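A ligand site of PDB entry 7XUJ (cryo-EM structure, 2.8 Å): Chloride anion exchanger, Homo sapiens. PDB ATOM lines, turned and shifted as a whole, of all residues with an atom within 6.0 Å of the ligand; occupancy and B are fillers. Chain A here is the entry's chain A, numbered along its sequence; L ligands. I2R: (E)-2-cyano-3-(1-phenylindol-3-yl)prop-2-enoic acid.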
ATOM      1  N   SER A  75      21.922  13.168  20.249  1.00  0.00           N
ATOM      2  CA  SER A  75      21.108  12.039  20.677  1.00  0.00           C
ATOM      3  C   SER A  75      21.928  10.955  21.376  1.00  0.00           C
ATOM      4  O   SER A  75      21.383  10.240  22.227  1.00  0.00           O
ATOM      5  CB  SER A  75      20.394  11.433  19.470  1.00  0.00           C
ATOM      6  OG  SER A  75      19.440  12.339  18.953  1.00  0.00           O
ATOM      7  N   VAL A  79      22.242  10.115  26.056  1.00  0.00           N
ATOM      8  CA  VAL A  79      22.300   8.719  26.486  1.00  0.00           C
ATOM      9  C   VAL A  79      23.622   8.421  27.175  1.00  0.00           C
ATOM     10  O   VAL A  79      23.655   7.660  28.156  1.00  0.00           O
ATOM     11  CB  VAL A  79      22.061   7.811  25.272  1.00  0.00           C
ATOM     12  CG1 VAL A  79      22.199   6.349  25.632  1.00  0.00           C
ATOM     13  CG2 VAL A  79      20.704   8.076  24.685  1.00  0.00           C
ATOM     14  N   LEU A  82      23.372   9.795  30.809  1.00  0.00           N
ATOM     15  CA  LEU A  82      22.547   8.960  31.695  1.00  0.00           C
ATOM     16  C   LEU A  82      23.190   7.603  31.959  1.00  0.00           C
ATOM     17  O   LEU A  82      23.136   7.099  33.084  1.00  0.00           O
ATOM     18  CB  LEU A  82      21.159   8.788  31.090  1.00  0.00           C
ATOM     19  CG  LEU A  82      20.322  10.051  31.046  1.00  0.00           C
ATOM     20  CD1 LEU A  82      18.928   9.727  30.546  1.00  0.00           C
ATOM     21  CD2 LEU A  82      20.256  10.701  32.406  1.00  0.00           C
ATOM     22  N   GLN A  83      23.831   7.028  30.951  1.00  0.00           N
ATOM     23  CA  GLN A  83      24.475   5.736  31.136  1.00  0.00           C
ATOM     24  C   GLN A  83      25.733   5.847  31.972  1.00  0.00           C
ATOM     25  O   GLN A  83      26.047   4.920  32.718  1.00  0.00           O
ATOM     26  CB  GLN A  83      24.806   5.118  29.788  1.00  0.00           C
ATOM     27  CG  GLN A  83      23.623   4.482  29.108  1.00  0.00           C
ATOM     28  CD  GLN A  83      24.044   3.548  28.007  1.00  0.00           C
ATOM     29  OE1 GLN A  83      25.190   3.120  27.945  1.00  0.00           O
ATOM     30  NE2 GLN A  83      23.106   3.210  27.139  1.00  0.00           N
ATOM     31  N   ALA A  86      24.472   6.009  35.504  1.00  0.00           N
ATOM     32  CA  ALA A  86      23.956   4.716  35.944  1.00  0.00           C
ATOM     33  C   ALA A  86      25.057   3.685  36.148  1.00  0.00           C
ATOM     34  O   ALA A  86      24.981   2.871  37.064  1.00  0.00           O
ATOM     35  CB  ALA A  86      22.933   4.193  34.953  1.00  0.00           C
ATOM     36  N   PHE A  87      26.095   3.695  35.308  1.00  0.00           N
ATOM     37  CA  PHE A  87      27.142   2.689  35.433  1.00  0.00           C
ATOM     38  C   PHE A  87      28.166   3.053  36.487  1.00  0.00           C
ATOM     39  O   PHE A  87      28.953   2.191  36.875  1.00  0.00           O
ATOM     40  CB  PHE A  87      27.861   2.466  34.104  1.00  0.00           C
ATOM     41  CG  PHE A  87      26.973   1.975  32.999  1.00  0.00           C
ATOM     42  CD1 PHE A  87      25.821   1.247  33.272  1.00  0.00           C
ATOM     43  CD2 PHE A  87      27.284   2.245  31.680  1.00  0.00           C
ATOM     44  CE1 PHE A  87      25.005   0.820  32.253  1.00  0.00           C
ATOM     45  CE2 PHE A  87      26.477   1.808  30.664  1.00  0.00           C
ATOM     46  CZ  PHE A  87      25.338   1.095  30.951  1.00  0.00           C
ATOM     47  N   PRO A 124      27.904  -2.003  30.987  1.00  0.00           N
ATOM     48  CA  PRO A 124      27.709  -2.491  32.370  1.00  0.00           C
ATOM     49  C   PRO A 124      28.492  -3.732  32.757  1.00  0.00           C
ATOM     50  O   PRO A 124      28.763  -3.916  33.947  1.00  0.00           O
ATOM     51  CB  PRO A 124      26.202  -2.742  32.437  1.00  0.00           C
ATOM     52  CG  PRO A 124      25.853  -3.065  31.077  1.00  0.00           C
ATOM     53  CD  PRO A 124      26.648  -2.148  30.228  1.00  0.00           C
ATOM     54  N   VAL A 214      24.067  -8.324  36.084  1.00  0.00           N
ATOM     55  CA  VAL A 214      23.638  -6.927  36.084  1.00  0.00           C
ATOM     56  C   VAL A 214      22.256  -6.779  36.703  1.00  0.00           C
ATOM     57  O   VAL A 214      22.022  -5.855  37.486  1.00  0.00           O
ATOM     58  CB  VAL A 214      23.694  -6.367  34.644  1.00  0.00           C
ATOM     59  CG1 VAL A 214      22.957  -5.053  34.526  1.00  0.00           C
ATOM     60  CG2 VAL A 214      25.117  -6.191  34.194  1.00  0.00           C
ATOM     61  N   LYS A 269       9.544   1.258  24.744  1.00  0.00           N
ATOM     62  CA  LYS A 269      10.567   0.643  23.905  1.00  0.00           C
ATOM     63  C   LYS A 269      10.021  -0.500  23.055  1.00  0.00           C
ATOM     64  O   LYS A 269      10.604  -0.795  22.007  1.00  0.00           O
ATOM     65  CB  LYS A 269      11.735   0.175  24.765  1.00  0.00           C
ATOM     66  CG  LYS A 269      12.738   1.269  25.055  1.00  0.00           C
ATOM     67  CD  LYS A 269      14.045   0.718  25.567  1.00  0.00           C
ATOM     68  CE  LYS A 269      14.831   0.047  24.451  1.00  0.00           C
ATOM     69  NZ  LYS A 269      16.152  -0.431  24.932  1.00  0.00           N
ATOM     70  N   ILE A 283      11.870   7.772  19.819  1.00  0.00           N
ATOM     71  CA  ILE A 283      11.425   8.475  21.014  1.00  0.00           C
ATOM     72  C   ILE A 283      12.450   8.335  22.128  1.00  0.00           C
ATOM     73  O   ILE A 283      12.752   7.204  22.555  1.00  0.00           O
ATOM     74  CB  ILE A 283      10.064   7.949  21.489  1.00  0.00           C
ATOM     75  CG1 ILE A 283       9.002   8.194  20.413  1.00  0.00           C
ATOM     76  CG2 ILE A 283       9.662   8.604  22.785  1.00  0.00           C
ATOM     77  CD1 ILE A 283       7.696   7.527  20.710  1.00  0.00           C
ATOM     78  N   PRO A 284      13.026   9.430  22.626  1.00  0.00           N
ATOM     79  CA  PRO A 284      13.945   9.329  23.767  1.00  0.00           C
ATOM     80  C   PRO A 284      13.164   9.222  25.073  1.00  0.00           C
ATOM     81  O   PRO A 284      13.022  10.199  25.813  1.00  0.00           O
ATOM     82  CB  PRO A 284      14.730  10.644  23.690  1.00  0.00           C
ATOM     83  CG  PRO A 284      14.276  11.325  22.420  1.00  0.00           C
ATOM     84  CD  PRO A 284      12.922  10.808  22.143  1.00  0.00           C
ATOM     85  N   ILE A 285      12.646   8.037  25.351  1.00  0.00           N
ATOM     86  CA  ILE A 285      11.796   7.825  26.521  1.00  0.00           C
ATOM     87  C   ILE A 285      12.594   7.841  27.802  1.00  0.00           C
ATOM     88  O   ILE A 285      12.071   8.234  28.859  1.00  0.00           O
ATOM     89  CB  ILE A 285      10.974   6.533  26.355  1.00  0.00           C
ATOM     90  CG1 ILE A 285       9.904   6.398  27.443  1.00  0.00           C
ATOM     91  CG2 ILE A 285      11.874   5.302  26.249  1.00  0.00           C
ATOM     92  CD1 ILE A 285       8.907   7.529  27.447  1.00  0.00           C
ATOM     93  N   GLU A 286      13.877   7.476  27.755  1.00  0.00           N
ATOM     94  CA  GLU A 286      14.699   7.488  28.949  1.00  0.00           C
ATOM     95  C   GLU A 286      15.057   8.902  29.376  1.00  0.00           C
ATOM     96  O   GLU A 286      15.020   9.216  30.575  1.00  0.00           O
ATOM     97  CB  GLU A 286      15.944   6.642  28.697  1.00  0.00           C
ATOM     98  CG  GLU A 286      15.664   5.191  28.968  1.00  0.00           C
ATOM     99  CD  GLU A 286      15.791   4.340  27.735  1.00  0.00           C
ATOM    100  OE1 GLU A 286      15.955   4.917  26.645  1.00  0.00           O
ATOM    101  OE2 GLU A 286      15.740   3.096  27.857  1.00  0.00           O
ATOM    102  N   ALA A 389      29.431   0.161  23.972  1.00  0.00           N
ATOM    103  CA  ALA A 389      28.220  -0.573  24.275  1.00  0.00           C
ATOM    104  C   ALA A 389      27.425  -0.774  22.991  1.00  0.00           C
ATOM    105  O   ALA A 389      27.448   0.087  22.106  1.00  0.00           O
ATOM    106  CB  ALA A 389      27.363   0.170  25.294  1.00  0.00           C
ATOM    107  N   SER A 391      24.160  -0.902  22.809  1.00  0.00           N
ATOM    108  CA  SER A 391      22.957  -0.079  22.849  1.00  0.00           C
ATOM    109  C   SER A 391      23.248   1.363  22.450  1.00  0.00           C
ATOM    110  O   SER A 391      22.519   1.959  21.654  1.00  0.00           O
ATOM    111  CB  SER A 391      22.348  -0.147  24.250  1.00  0.00           C
ATOM    112  OG  SER A 391      22.074  -1.488  24.607  1.00  0.00           O
ATOM    113  N   ARG A 392      24.326   1.942  23.002  1.00  0.00           N
ATOM    114  CA  ARG A 392      24.657   3.329  22.686  1.00  0.00           C
ATOM    115  C   ARG A 392      25.159   3.454  21.252  1.00  0.00           C
ATOM    116  O   ARG A 392      24.878   4.466  20.588  1.00  0.00           O
ATOM    117  CB  ARG A 392      25.709   3.836  23.669  1.00  0.00           C
ATOM    118  CG  ARG A 392      25.648   5.322  23.918  1.00  0.00           C
ATOM    119  CD  ARG A 392      26.891   5.809  24.639  1.00  0.00           C
ATOM    120  NE  ARG A 392      27.268   4.954  25.760  1.00  0.00           N
ATOM    121  CZ  ARG A 392      28.389   4.257  25.830  1.00  0.00           C
ATOM    122  NH1 ARG A 392      29.246   4.297  24.825  1.00  0.00           N
ATOM    123  NH2 ARG A 392      28.640   3.510  26.879  1.00  0.00           N
ATOM    124  N   SER A 393      25.880   2.456  20.760  1.00  0.00           N
ATOM    125  CA  SER A 393      26.292   2.452  19.365  1.00  0.00           C
ATOM    126  C   SER A 393      25.106   2.319  18.432  1.00  0.00           C
ATOM    127  O   SER A 393      25.082   2.925  17.361  1.00  0.00           O
ATOM    128  CB  SER A 393      27.280   1.316  19.105  1.00  0.00           C
ATOM    129  OG  SER A 393      28.429   1.467  19.916  1.00  0.00           O
ATOM    130  N   VAL A 395      22.143   3.501  19.157  1.00  0.00           N
ATOM    131  CA  VAL A 395      21.507   4.816  19.189  1.00  0.00           C
ATOM    132  C   VAL A 395      22.244   5.800  18.286  1.00  0.00           C
ATOM    133  O   VAL A 395      21.615   6.577  17.548  1.00  0.00           O
ATOM    134  CB  VAL A 395      21.436   5.323  20.650  1.00  0.00           C
ATOM    135  CG1 VAL A 395      21.016   6.777  20.712  1.00  0.00           C
ATOM    136  CG2 VAL A 395      20.463   4.497  21.429  1.00  0.00           C
ATOM    137  N   LEU A 433      17.724   5.440  37.807  1.00  0.00           N
ATOM    138  CA  LEU A 433      18.854   4.987  37.012  1.00  0.00           C
ATOM    139  C   LEU A 433      18.937   3.464  36.970  1.00  0.00           C
ATOM    140  O   LEU A 433      19.243   2.883  35.924  1.00  0.00           O
ATOM    141  CB  LEU A 433      20.144   5.577  37.568  1.00  0.00           C
ATOM    142  CG  LEU A 433      20.247   7.102  37.535  1.00  0.00           C
ATOM    143  CD1 LEU A 433      21.468   7.554  38.273  1.00  0.00           C
ATOM    144  CD2 LEU A 433      20.277   7.583  36.108  1.00  0.00           C
ATOM    145  N   LEU A 436      16.261   2.337  34.613  1.00  0.00           N
ATOM    146  CA  LEU A 436      16.672   2.539  33.223  1.00  0.00           C
ATOM    147  C   LEU A 436      17.675   1.493  32.785  1.00  0.00           C
ATOM    148  O   LEU A 436      17.674   1.067  31.624  1.00  0.00           O
ATOM    149  CB  LEU A 436      17.265   3.931  33.038  1.00  0.00           C
ATOM    150  CG  LEU A 436      16.356   5.147  33.161  1.00  0.00           C
ATOM    151  CD1 LEU A 436      17.012   6.360  32.544  1.00  0.00           C
ATOM    152  CD2 LEU A 436      14.992   4.900  32.562  1.00  0.00           C
ATOM    153  N   ALA A 437      18.547   1.053  33.698  1.00  0.00           N
ATOM    154  CA  ALA A 437      19.485   0.002  33.345  1.00  0.00           C
ATOM    155  C   ALA A 437      18.794  -1.364  33.258  1.00  0.00           C
ATOM    156  O   ALA A 437      19.216  -2.211  32.479  1.00  0.00           O
ATOM    157  CB  ALA A 437      20.630  -0.051  34.346  1.00  0.00           C
ATOM    158  N   LEU A 438      17.745  -1.576  34.050  1.00  0.00           N
ATOM    159  CA  LEU A 438      17.012  -2.846  33.952  1.00  0.00           C
ATOM    160  C   LEU A 438      16.096  -2.888  32.748  1.00  0.00           C
ATOM    161  O   LEU A 438      15.772  -3.982  32.266  1.00  0.00           O
ATOM    162  CB  LEU A 438      16.195  -3.090  35.208  1.00  0.00           C
ATOM    163  CG  LEU A 438      16.920  -3.543  36.467  1.00  0.00           C
ATOM    164  CD1 LEU A 438      15.924  -4.016  37.475  1.00  0.00           C
ATOM    165  CD2 LEU A 438      17.918  -4.626  36.152  1.00  0.00           C
ATOM    166  N   GLY A 439      15.659  -1.735  32.251  1.00  0.00           N
ATOM    167  CA  GLY A 439      14.771  -1.735  31.103  1.00  0.00           C
ATOM    168  C   GLY A 439      15.421  -2.066  29.791  1.00  0.00           C
ATOM    169  O   GLY A 439      14.724  -2.185  28.777  1.00  0.00           O
ATOM    170  N   ASN A 440      16.745  -2.220  29.764  1.00  0.00           N
ATOM    171  CA  ASN A 440      17.469  -2.461  28.527  1.00  0.00           C
ATOM    172  C   ASN A 440      18.322  -3.712  28.630  1.00  0.00           C
ATOM    173  O   ASN A 440      19.326  -3.850  27.928  1.00  0.00           O
ATOM    174  CB  ASN A 440      18.304  -1.257  28.154  1.00  0.00           C
ATOM    175  CG  ASN A 440      17.487   0.014  28.104  1.00  0.00           C
ATOM    176  OD1 ASN A 440      16.983   0.407  27.051  1.00  0.00           O
ATOM    177  ND2 ASN A 440      17.358   0.697  29.242  1.00  0.00           N
ATOM    178  N   LEU A 441      17.941  -4.633  29.502  1.00  0.00           N
ATOM    179  CA  LEU A 441      18.520  -5.967  29.548  1.00  0.00           C
ATOM    180  C   LEU A 441      17.766  -6.959  28.693  1.00  0.00           C
ATOM    181  O   LEU A 441      18.067  -8.154  28.746  1.00  0.00           O
ATOM    182  CB  LEU A 441      18.549  -6.477  30.991  1.00  0.00           C
ATOM    183  CG  LEU A 441      19.594  -5.899  31.935  1.00  0.00           C
ATOM    184  CD1 LEU A 441      19.433  -6.545  33.280  1.00  0.00           C
ATOM    185  CD2 LEU A 441      20.974  -6.125  31.391  1.00  0.00           C
ATOM    186  N   MET A 444      19.834  -8.925  25.867  1.00  0.00           N
ATOM    187  CA  MET A 444      20.745  -9.947  26.359  1.00  0.00           C
ATOM    188  C   MET A 444      20.001 -11.077  27.061  1.00  0.00           C
ATOM    189  O   MET A 444      20.497 -12.204  27.098  1.00  0.00           O
ATOM    190  CB  MET A 444      21.773  -9.330  27.290  1.00  0.00           C
ATOM    191  CG  MET A 444      22.901  -8.627  26.576  1.00  0.00           C
ATOM    192  SD  MET A 444      24.272  -8.235  27.668  1.00  0.00           S
ATOM    193  CE  MET A 444      23.553  -6.954  28.674  1.00  0.00           C
HETATM  194  C10 I2R L   1      21.317   2.449  31.170  1.00  0.00           C
HETATM  195  C13 I2R L   1      21.040   3.714  31.908  1.00  0.00           C
HETATM  196  C15 I2R L   1      21.262  -0.903  30.215  1.00  0.00           C
HETATM  197  C17 I2R L   1      21.896  -2.283  30.370  1.00  0.00           C
HETATM  198  C20 I2R L   1      22.816  -2.823  29.275  1.00  0.00           C
HETATM  199  C21 I2R L   1      18.318   4.680  24.669  1.00  0.00           C
HETATM  200  C22 I2R L   1      20.558   3.407  24.923  1.00  0.00           C
HETATM  201  C5  I2R L   1      20.812   2.257  29.710  1.00  0.00           C
HETATM  202  C6  I2R L   1      20.094   3.284  29.098  1.00  0.00           C
HETATM  203  C7  I2R L   1      19.777   2.886  27.852  1.00  0.00           C
HETATM  204  C8  I2R L   1      20.285   1.608  27.678  1.00  0.00           C
HETATM  205  C9  I2R L   1      21.550  -0.057  28.983  1.00  0.00           C
HETATM  206  C11 I2R L   1      19.794   4.622  29.853  1.00  0.00           C
HETATM  207  C12 I2R L   1      18.967   3.672  26.816  1.00  0.00           C
HETATM  208  C14 I2R L   1      20.284   4.802  31.254  1.00  0.00           C
HETATM  209  C16 I2R L   1      22.460  -0.597  27.888  1.00  0.00           C
HETATM  210  C18 I2R L   1      23.103  -1.971  28.030  1.00  0.00           C
HETATM  211  C19 I2R L   1      19.256   3.886  25.543  1.00  0.00           C
HETATM  212  N3  I2R L   1      20.918   1.232  28.819  1.00  0.00           N
HETATM  213  N4  I2R L   1      21.529   3.051  24.452  1.00  0.00           N
HETATM  214  O1  I2R L   1      17.668   4.085  23.796  1.00  0.00           O
HETATM  215  O2  I2R L   1      18.194   5.907  24.800  1.00  0.00           O
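N4 of the ligand sits close to O of Ser 391, 3.2 Å away. Val 79 touches the ligand. CB of Ala 86 touches C13 of the ligand, at 3.6 Å. Pro 124 touches the ligand (CG to C20, 3.5 Å). Val 395 touches the ligand (CG2 to N4, 3.5 Å). CB of Leu 436 touches C14 of the ligand, at 3.6 Å. Ala 437 touches the ligand. CG of Asn 440 touches C8 of the ligand (3.2 Å). Of the 26 residues printed, 11 come within 4 Å of the ligand. The nearest printed residue that does not touch the ligand is Leu 441 (4.1 Å).
An oxygen (O2) of the ligand sits close to the side-chain carboxylate (OE1) of Glu 286, at 3.1 Å. A nitrogen (N4) of the ligand lies within hydrogen-bond range of the side-chain amide nitrogen (NE2) of Gln 83 (3.1 Å). The backbone NH (N) of Arg 392 sits at hydrogen-bond distance from a nitrogen (N4) of the ligand, at 3.3 Å.
OE2 of Glu 286 sits close to OD1 of Asn 440 (3.1 Å). OD1 of Asn 440 sits at hydrogen-bond distance from NZ of Lys 269, 2.4 Å away. The side-chain amide nitrogen (ND2) of Asn 440 sits at hydrogen-bond distance from the backbone carbonyl oxygen (O) of Leu 436 (2.4 Å).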
